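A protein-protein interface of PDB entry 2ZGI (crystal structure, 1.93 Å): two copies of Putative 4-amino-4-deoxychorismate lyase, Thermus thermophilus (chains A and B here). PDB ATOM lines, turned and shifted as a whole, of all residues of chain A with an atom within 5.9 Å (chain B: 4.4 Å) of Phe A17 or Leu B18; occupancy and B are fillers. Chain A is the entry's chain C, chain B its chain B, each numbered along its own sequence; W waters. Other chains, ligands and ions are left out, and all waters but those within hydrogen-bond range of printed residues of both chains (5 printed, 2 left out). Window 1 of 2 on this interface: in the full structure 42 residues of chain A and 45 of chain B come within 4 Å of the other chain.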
ATOM      1  N   LEU A  13      -7.720  16.576  17.218  1.00  0.00           N
ATOM      2  CA  LEU A  13      -6.952  17.283  16.208  1.00  0.00           C
ATOM      3  C   LEU A  13      -7.016  18.795  16.421  1.00  0.00           C
ATOM      4  O   LEU A  13      -7.983  19.298  17.011  1.00  0.00           O
ATOM      5  CB  LEU A  13      -7.429  16.884  14.817  1.00  0.00           C
ATOM      6  CG  LEU A  13      -7.095  15.448  14.412  1.00  0.00           C
ATOM      7  CD1 LEU A  13      -8.180  14.865  13.557  1.00  0.00           C
ATOM      8  CD2 LEU A  13      -5.754  15.332  13.709  1.00  0.00           C
ATOM      9  N   PRO A  14      -5.973  19.530  15.967  1.00  0.00           N
ATOM     10  CA  PRO A  14      -6.081  20.956  16.139  1.00  0.00           C
ATOM     11  C   PRO A  14      -7.158  21.503  15.229  1.00  0.00           C
ATOM     12  O   PRO A  14      -7.401  20.978  14.128  1.00  0.00           O
ATOM     13  CB  PRO A  14      -4.708  21.478  15.703  1.00  0.00           C
ATOM     14  CG  PRO A  14      -3.834  20.284  15.630  1.00  0.00           C
ATOM     15  CD  PRO A  14      -4.734  19.173  15.263  1.00  0.00           C
ATOM     16  N   GLU A  15      -7.794  22.552  15.711  1.00  0.00           N
ATOM     17  CA  GLU A  15      -8.821  23.272  14.982  1.00  0.00           C
ATOM     18  C   GLU A  15      -8.474  23.621  13.514  1.00  0.00           C
ATOM     19  O   GLU A  15      -9.297  23.402  12.618  1.00  0.00           O
ATOM     20  CB  GLU A  15      -9.108  24.532  15.768  1.00  0.00           C
ATOM     21  CG  GLU A  15     -10.299  25.272  15.338  1.00  0.00           C
ATOM     22  CD  GLU A  15     -10.632  26.358  16.320  1.00  0.00           C
ATOM     23  OE1 GLU A  15     -10.807  26.015  17.516  1.00  0.00           O
ATOM     24  OE2 GLU A  15     -10.712  27.534  15.885  1.00  0.00           O
ATOM     25  N   ALA A  16      -7.276  24.153  13.267  1.00  0.00           N
ATOM     26  CA  ALA A  16      -6.869  24.526  11.898  1.00  0.00           C
ATOM     27  C   ALA A  16      -6.955  23.362  10.907  1.00  0.00           C
ATOM     28  O   ALA A  16      -7.370  23.535   9.746  1.00  0.00           O
ATOM     29  CB  ALA A  16      -5.449  25.112  11.879  1.00  0.00           C
ATOM     30  N   PHE A  17      -6.528  22.186  11.360  1.00  0.00           N
ATOM     31  CA  PHE A  17      -6.499  20.986  10.513  1.00  0.00           C
ATOM     32  C   PHE A  17      -7.925  20.640  10.128  1.00  0.00           C
ATOM     33  O   PHE A  17      -8.218  20.325   8.961  1.00  0.00           O
ATOM     34  CB  PHE A  17      -5.840  19.807  11.245  1.00  0.00           C
ATOM     35  CG  PHE A  17      -5.718  18.549  10.394  1.00  0.00           C
ATOM     36  CD1 PHE A  17      -4.570  18.308   9.667  1.00  0.00           C
ATOM     37  CD2 PHE A  17      -6.769  17.629  10.304  1.00  0.00           C
ATOM     38  CE1 PHE A  17      -4.435  17.136   8.871  1.00  0.00           C
ATOM     39  CE2 PHE A  17      -6.655  16.479   9.499  1.00  0.00           C
ATOM     40  CZ  PHE A  17      -5.473  16.236   8.782  1.00  0.00           C
ATOM     41  N   LEU A  18      -8.808  20.742  11.123  1.00  0.00           N
ATOM     42  CA  LEU A  18     -10.184  20.269  11.031  1.00  0.00           C
ATOM     43  C   LEU A  18     -11.109  21.301  10.412  1.00  0.00           C
ATOM     44  O   LEU A  18     -11.877  21.008   9.480  1.00  0.00           O
ATOM     45  CB  LEU A  18     -10.668  19.945  12.462  1.00  0.00           C
ATOM     46  CG  LEU A  18     -11.672  18.829  12.759  1.00  0.00           C
ATOM     47  CD1 LEU A  18     -11.503  17.587  11.855  1.00  0.00           C
ATOM     48  CD2 LEU A  18     -11.509  18.408  14.221  1.00  0.00           C
ATOM     49  N   TYR A  19     -11.053  22.521  10.922  1.00  0.00           N
ATOM     50  CA  TYR A  19     -12.036  23.499  10.487  1.00  0.00           C
ATOM     51  C   TYR A  19     -11.664  24.198   9.180  1.00  0.00           C
ATOM     52  O   TYR A  19     -12.527  24.715   8.489  1.00  0.00           O
ATOM     53  CB  TYR A  19     -12.324  24.512  11.583  1.00  0.00           C
ATOM     54  CG  TYR A  19     -13.037  23.955  12.820  1.00  0.00           C
ATOM     55  CD1 TYR A  19     -13.530  22.647  12.865  1.00  0.00           C
ATOM     56  CD2 TYR A  19     -13.225  24.750  13.922  1.00  0.00           C
ATOM     57  CE1 TYR A  19     -14.173  22.157  14.026  1.00  0.00           C
ATOM     58  CE2 TYR A  19     -13.863  24.295  15.051  1.00  0.00           C
ATOM     59  CZ  TYR A  19     -14.330  23.011  15.112  1.00  0.00           C
ATOM     60  OH  TYR A  19     -14.952  22.600  16.267  1.00  0.00           O
ATOM     61  N   HIS A  20     -10.381  24.199   8.857  1.00  0.00           N
ATOM     62  CA  HIS A  20      -9.869  25.075   7.800  1.00  0.00           C
ATOM     63  C   HIS A  20      -9.182  24.344   6.658  1.00  0.00           C
ATOM     64  O   HIS A  20      -8.631  24.981   5.755  1.00  0.00           O
ATOM     65  CB  HIS A  20      -8.886  26.061   8.418  1.00  0.00           C
ATOM     66  CG  HIS A  20      -9.516  27.019   9.370  1.00  0.00           C
ATOM     67  ND1 HIS A  20      -8.776  27.783  10.253  1.00  0.00           N
ATOM     68  CD2 HIS A  20     -10.815  27.333   9.591  1.00  0.00           C
ATOM     69  CE1 HIS A  20      -9.598  28.527  10.971  1.00  0.00           C
ATOM     70  NE2 HIS A  20     -10.836  28.273  10.592  1.00  0.00           N
ATOM     71  N   GLY A  21      -9.199  23.009   6.713  1.00  0.00           N
ATOM     72  CA  GLY A  21      -8.623  22.199   5.666  1.00  0.00           C
ATOM     73  C   GLY A  21      -7.117  22.450   5.591  1.00  0.00           C
ATOM     74  O   GLY A  21      -6.538  22.351   4.541  1.00  0.00           O
ATOM     75  N   ALA A  22      -6.514  22.827   6.718  1.00  0.00           N
ATOM     76  CA  ALA A  22      -5.106  23.242   6.764  1.00  0.00           C
ATOM     77  C   ALA A  22      -4.160  22.045   6.823  1.00  0.00           C
ATOM     78  O   ALA A  22      -3.613  21.716   7.899  1.00  0.00           O
ATOM     79  CB  ALA A  22      -4.862  24.176   7.971  1.00  0.00           C
ATOM     80  N   SER A  23      -3.939  21.426   5.656  1.00  0.00           N
ATOM     81  CA  SER A  23      -3.109  20.224   5.514  1.00  0.00           C
ATOM     82  C   SER A  23      -2.671  20.069   4.076  1.00  0.00           C
ATOM     83  O   SER A  23      -3.310  20.609   3.161  1.00  0.00           O
ATOM     84  CB  SER A  23      -3.909  18.973   5.946  1.00  0.00           C
ATOM     85  OG  SER A  23      -5.122  18.821   5.212  1.00  0.00           O
ATOM     86  N   THR A  84      -0.769  12.414   5.415  1.00  0.00           N
ATOM     87  CA  THR A  84      -1.324  13.752   5.526  1.00  0.00           C
ATOM     88  C   THR A  84      -0.495  14.492   6.578  1.00  0.00           C
ATOM     89  O   THR A  84      -0.158  13.938   7.628  1.00  0.00           O
ATOM     90  CB  THR A  84      -2.806  13.689   5.915  1.00  0.00           C
ATOM     91  OG1 THR A  84      -3.518  12.862   4.970  1.00  0.00           O
ATOM     92  CG2 THR A  84      -3.447  15.084   5.924  1.00  0.00           C
ATOM     93  N   VAL A  85      -0.182  15.748   6.287  1.00  0.00           N
ATOM     94  CA  VAL A  85       0.576  16.597   7.194  1.00  0.00           C
ATOM     95  C   VAL A  85      -0.226  17.863   7.508  1.00  0.00           C
ATOM     96  O   VAL A  85      -0.665  18.558   6.592  1.00  0.00           O
ATOM     97  CB  VAL A  85       1.945  17.024   6.522  1.00  0.00           C
ATOM     98  CG1 VAL A  85       2.688  18.055   7.400  1.00  0.00           C
ATOM     99  CG2 VAL A  85       2.839  15.817   6.296  1.00  0.00           C
ATOM    100  N   GLY A  86      -0.414  18.151   8.796  1.00  0.00           N
ATOM    101  CA  GLY A  86      -0.858  19.459   9.253  1.00  0.00           C
ATOM    102  C   GLY A  86      -0.017  19.848  10.450  1.00  0.00           C
ATOM    103  O   GLY A  86       0.794  19.029  10.921  1.00  0.00           O
ATOM    104  N   GLU A  87      -0.211  21.058  10.974  1.00  0.00           N
ATOM    105  CA  GLU A  87       0.540  21.504  12.167  1.00  0.00           C
ATOM    106  C   GLU A  87       0.206  20.667  13.406  1.00  0.00           C
ATOM    107  O   GLU A  87      -0.923  20.622  13.825  1.00  0.00           O
ATOM    108  CB  GLU A  87       0.257  22.969  12.447  1.00  0.00           C
ATOM    109  CG  GLU A  87       1.182  23.896  11.692  1.00  0.00           C
ATOM    110  CD  GLU A  87       2.640  23.676  12.051  1.00  0.00           C
ATOM    111  OE1 GLU A  87       2.941  23.571  13.257  1.00  0.00           O
ATOM    112  OE2 GLU A  87       3.481  23.615  11.130  1.00  0.00           O
ATOM    113  N   VAL A  89       0.186  17.491  13.394  1.00  0.00           N
ATOM    114  CA  VAL A  89      -0.527  16.323  12.888  1.00  0.00           C
ATOM    115  C   VAL A  89       0.267  15.589  11.816  1.00  0.00           C
ATOM    116  O   VAL A  89       0.539  16.139  10.758  1.00  0.00           O
ATOM    117  CB  VAL A  89      -1.893  16.712  12.247  1.00  0.00           C
ATOM    118  CG1 VAL A  89      -2.554  15.503  11.632  1.00  0.00           C
ATOM    119  CG2 VAL A  89      -2.808  17.307  13.261  1.00  0.00           C
ATOM    120  N   LEU A  91      -0.719  12.176   9.901  1.00  0.00           N
ATOM    121  CA  LEU A  91      -1.822  11.227   9.788  1.00  0.00           C
ATOM    122  C   LEU A  91      -1.518  10.292   8.639  1.00  0.00           C
ATOM    123  O   LEU A  91      -1.253  10.735   7.516  1.00  0.00           O
ATOM    124  CB  LEU A  91      -3.135  12.006   9.604  1.00  0.00           C
ATOM    125  CG  LEU A  91      -4.517  11.587  10.109  1.00  0.00           C
ATOM    126  CD1 LEU A  91      -4.500  10.469  11.119  1.00  0.00           C
ATOM    127  CD2 LEU A  91      -5.272  12.811  10.650  1.00  0.00           C
ATOM    128  N   GLU A  93      -2.836   6.595   6.867  1.00  0.00           N
ATOM    129  CA  GLU A  93      -3.913   5.607   6.812  1.00  0.00           C
ATOM    130  C   GLU A  93      -3.854   4.692   5.586  1.00  0.00           C
ATOM    131  O   GLU A  93      -3.183   4.994   4.564  1.00  0.00           O
ATOM    132  CB  GLU A  93      -5.310   6.242   6.997  1.00  0.00           C
ATOM    133  CG  GLU A  93      -5.740   7.230   5.894  1.00  0.00           C
ATOM    134  CD  GLU A  93      -7.258   7.430   5.818  1.00  0.00           C
ATOM    135  OE1 GLU A  93      -7.787   7.312   4.700  1.00  0.00           O
ATOM    136  OE2 GLU A  93      -7.924   7.709   6.850  1.00  0.00           O
ATOM    137  N   ARG B   2      -6.426   4.195  10.488  1.00  0.00           N
ATOM    138  CA  ARG B   2      -5.752   5.491  10.676  1.00  0.00           C
ATOM    139  C   ARG B   2      -4.736   5.454  11.815  1.00  0.00           C
ATOM    140  O   ARG B   2      -5.054   4.953  12.893  1.00  0.00           O
ATOM    141  CB  ARG B   2      -6.756   6.593  11.044  1.00  0.00           C
ATOM    142  CG  ARG B   2      -7.701   7.031   9.957  1.00  0.00           C
ATOM    143  CD  ARG B   2      -8.657   8.091  10.467  1.00  0.00           C
ATOM    144  NE  ARG B   2      -9.663   8.423   9.461  1.00  0.00           N
ATOM    145  CZ  ARG B   2     -10.836   8.994   9.722  1.00  0.00           C
ATOM    146  NH1 ARG B   2     -11.174   9.295  10.975  1.00  0.00           N
ATOM    147  NH2 ARG B   2     -11.675   9.265   8.724  1.00  0.00           N
ATOM    148  N   PRO B  14     -15.852  11.891   9.746  1.00  0.00           N
ATOM    149  CA  PRO B  14     -15.804  11.329   8.399  1.00  0.00           C
ATOM    150  C   PRO B  14     -14.675  11.959   7.564  1.00  0.00           C
ATOM    151  O   PRO B  14     -14.317  13.123   7.809  1.00  0.00           O
ATOM    152  CB  PRO B  14     -17.171  11.694   7.807  1.00  0.00           C
ATOM    153  CG  PRO B  14     -18.010  12.154   8.961  1.00  0.00           C
ATOM    154  CD  PRO B  14     -17.061  12.698   9.969  1.00  0.00           C
ATOM    155  N   GLU B  15     -14.145  11.173   6.616  1.00  0.00           N
ATOM    156  CA  GLU B  15     -13.036  11.566   5.714  1.00  0.00           C
ATOM    157  C   GLU B  15     -13.218  12.960   5.100  1.00  0.00           C
ATOM    158  O   GLU B  15     -12.320  13.788   5.183  1.00  0.00           O
ATOM    159  CB  GLU B  15     -12.835  10.531   4.585  1.00  0.00           C
ATOM    160  CG  GLU B  15     -11.753  10.901   3.539  1.00  0.00           C
ATOM    161  CD  GLU B  15     -11.548   9.864   2.426  1.00  0.00           C
ATOM    162  OE1 GLU B  15     -11.384   8.657   2.725  1.00  0.00           O
ATOM    163  OE2 GLU B  15     -11.524  10.269   1.237  1.00  0.00           O
ATOM    164  N   ALA B  16     -14.357  13.192   4.459  1.00  0.00           N
ATOM    165  CA  ALA B  16     -14.590  14.472   3.759  1.00  0.00           C
ATOM    166  C   ALA B  16     -14.449  15.673   4.723  1.00  0.00           C
ATOM    167  O   ALA B  16     -13.738  16.647   4.408  1.00  0.00           O
ATOM    168  CB  ALA B  16     -15.934  14.489   3.084  1.00  0.00           C
ATOM    169  N   PHE B  17     -15.057  15.564   5.908  1.00  0.00           N
ATOM    170  CA  PHE B  17     -14.965  16.641   6.900  1.00  0.00           C
ATOM    171  C   PHE B  17     -13.510  16.820   7.342  1.00  0.00           C
ATOM    172  O   PHE B  17     -13.010  17.957   7.453  1.00  0.00           O
ATOM    173  CB  PHE B  17     -15.864  16.367   8.120  1.00  0.00           C
ATOM    174  CG  PHE B  17     -15.887  17.488   9.112  1.00  0.00           C
ATOM    175  CD1 PHE B  17     -16.729  18.574   8.933  1.00  0.00           C
ATOM    176  CD2 PHE B  17     -15.066  17.460  10.231  1.00  0.00           C
ATOM    177  CE1 PHE B  17     -16.739  19.630   9.853  1.00  0.00           C
ATOM    178  CE2 PHE B  17     -15.055  18.507  11.141  1.00  0.00           C
ATOM    179  CZ  PHE B  17     -15.892  19.589  10.953  1.00  0.00           C
ATOM    180  N   LEU B  18     -12.837  15.687   7.562  1.00  0.00           N
ATOM    181  CA  LEU B  18     -11.513  15.661   8.173  1.00  0.00           C
ATOM    182  C   LEU B  18     -10.374  16.102   7.216  1.00  0.00           C
ATOM    183  O   LEU B  18      -9.451  16.804   7.623  1.00  0.00           O
ATOM    184  CB  LEU B  18     -11.242  14.243   8.685  1.00  0.00           C
ATOM    185  CG  LEU B  18      -9.861  13.797   9.180  1.00  0.00           C
ATOM    186  CD1 LEU B  18      -9.503  14.471  10.489  1.00  0.00           C
ATOM    187  CD2 LEU B  18      -9.817  12.297   9.375  1.00  0.00           C
ATOM    188  N   TYR B  19     -10.454  15.663   5.967  1.00  0.00           N
ATOM    189  CA  TYR B  19      -9.343  15.787   5.034  1.00  0.00           C
ATOM    190  C   TYR B  19      -9.610  16.797   3.936  1.00  0.00           C
ATOM    191  O   TYR B  19      -8.676  17.218   3.264  1.00  0.00           O
ATOM    192  CB  TYR B  19      -9.070  14.442   4.337  1.00  0.00           C
ATOM    193  CG  TYR B  19      -8.453  13.359   5.203  1.00  0.00           C
ATOM    194  CD1 TYR B  19      -7.391  13.637   6.051  1.00  0.00           C
ATOM    195  CD2 TYR B  19      -8.894  12.045   5.115  1.00  0.00           C
ATOM    196  CE1 TYR B  19      -6.808  12.634   6.837  1.00  0.00           C
ATOM    197  CE2 TYR B  19      -8.324  11.038   5.889  1.00  0.00           C
ATOM    198  CZ  TYR B  19      -7.290  11.341   6.751  1.00  0.00           C
ATOM    199  OH  TYR B  19      -6.703  10.363   7.519  1.00  0.00           O
ATOM    200  N   HIS B  20     -10.869  17.138   3.711  1.00  0.00           N
ATOM    201  CA  HIS B  20     -11.218  17.894   2.501  1.00  0.00           C
ATOM    202  C   HIS B  20     -11.815  19.273   2.771  1.00  0.00           C
ATOM    203  O   HIS B  20     -12.173  19.984   1.832  1.00  0.00           O
ATOM    204  CB  HIS B  20     -12.139  17.070   1.607  1.00  0.00           C
ATOM    205  CG  HIS B  20     -11.498  15.832   1.082  1.00  0.00           C
ATOM    206  ND1 HIS B  20     -12.222  14.780   0.560  1.00  0.00           N
ATOM    207  CD2 HIS B  20     -10.194  15.479   0.984  1.00  0.00           C
ATOM    208  CE1 HIS B  20     -11.390  13.830   0.181  1.00  0.00           C
ATOM    209  NE2 HIS B  20     -10.157  14.226   0.437  1.00  0.00           N
HETATM  210  O   HOH W   1      -7.399  18.933   6.651  1.00  0.00           O
HETATM  211  O   HOH W   2      -3.807  10.301   6.165  1.00  0.00           O
HETATM  212  O   HOH W   3     -13.967  20.796   7.546  1.00  0.00           O
HETATM  213  O   HOH W   4      -5.896  16.588   3.517  1.00  0.00           O
HETATM  214  O   HOH W   5     -11.064   8.103   5.066  1.00  0.00           O
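Of the printed residues of chain B, Phe A17 touches Leu B18 (3.4 Å).
Leu B18 touches three residues of chain A.
Printed residues of chain B within 4 Å of Leu A13: Leu B18.
Of the printed residues of chain A, Tyr B19 touches Thr A84, Leu A91 and Glu A93.
Of the printed residues of chain B, Glu A93 touches Arg B2 (3.2 Å) and Tyr B19 (3.0 Å).
Of the printed residues of chain A, Arg B2 touches Glu A93 (3.2 Å).
Printed residues of chain B within 4 Å of Thr A84: Tyr B19 (3.8 Å).
Val A85 touches none of the printed residues of chain B.
The nearest residue of chain A that does not touch Leu B18 is Leu A91 (4.5 Å).
Phe A17 touches Leu B18, and with the chains exchanged Leu A18 touches Phe B17.
Leu A18 touches its own counterpart, Leu B18.
7 positions are printed for both chains.
Leu A13 touches Leu B18.
Leu B18 touches Phe A17.
Leu A18 touches Phe B17 (CD1 to CE2, 3.7 Å).
CD1 of Leu A18 touches CD1 of Leu B18 (3.9 Å).
OG1 of Thr A84 touches CE1 of Tyr B19, at 3.8 Å.
OH of Tyr B19 touches CG of Leu A91, 3.6 Å away.
The side-chain carboxylate of Glu A93 is in salt-bridge range of the guanidinium group of Arg B2 (3.2 Å).
The side-chain hydroxyl (OH) of Tyr B19 lies within hydrogen-bond range of the side-chain carboxylate (OE2) of Glu A93 (3.0 Å).
Water W5 lies within hydrogen-bond range of the side-chain carboxylate (OE1) of Glu B15 (2.4 Å) and the side-chain carboxylate (OE1) of Glu A93 (3.4 Å).
Water W1 lies within hydrogen-bond range of the side-chain hydroxyl of Ser A23, the backbone carbonyl oxygen of Phe A17 and the backbone carbonyl oxygen of Leu B18.
Water W2 lies within hydrogen-bond range of the side-chain hydroxyl of Thr A84 (2.8 Å), the backbone carbonyl oxygen of Leu A91 (2.9 Å) and the side-chain hydroxyl of Tyr B19 (3.2 Å).
Water W3 bridges the backbone carbonyl oxygen (O) of Leu A18 (2.9 Å) and the backbone carbonyl oxygen (O) of Phe B17 (3.0 Å).
Water W4 lies within hydrogen-bond range of O of Tyr B19 and OG of Ser A23.
O of Leu A91 sits at hydrogen-bond distance from N of Thr A84.
Of the 8 printed residues of chain B, 4 touch a printed residue of chain A.
Printed residues of chain B that touch a printed residue of chain A: Arg B2, Phe B17, Leu B18 and Tyr B19.
Along chain B the printed residues that touch a printed residue of chain A span positions 2 to 19.
Of the 18 printed residues of chain A, 6 touch a printed residue of chain B.
Hydrophobic or aromatic side chains of chain A within 4 Å of the printed part of chain B: Leu A13, Phe A17, Leu A18 and Leu A91.
Among the printed residues, Asp or Glu carboxylates within 4 Å of a Lys or Arg side-chain nitrogen of the other chain: Glu A93 with Arg B2.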
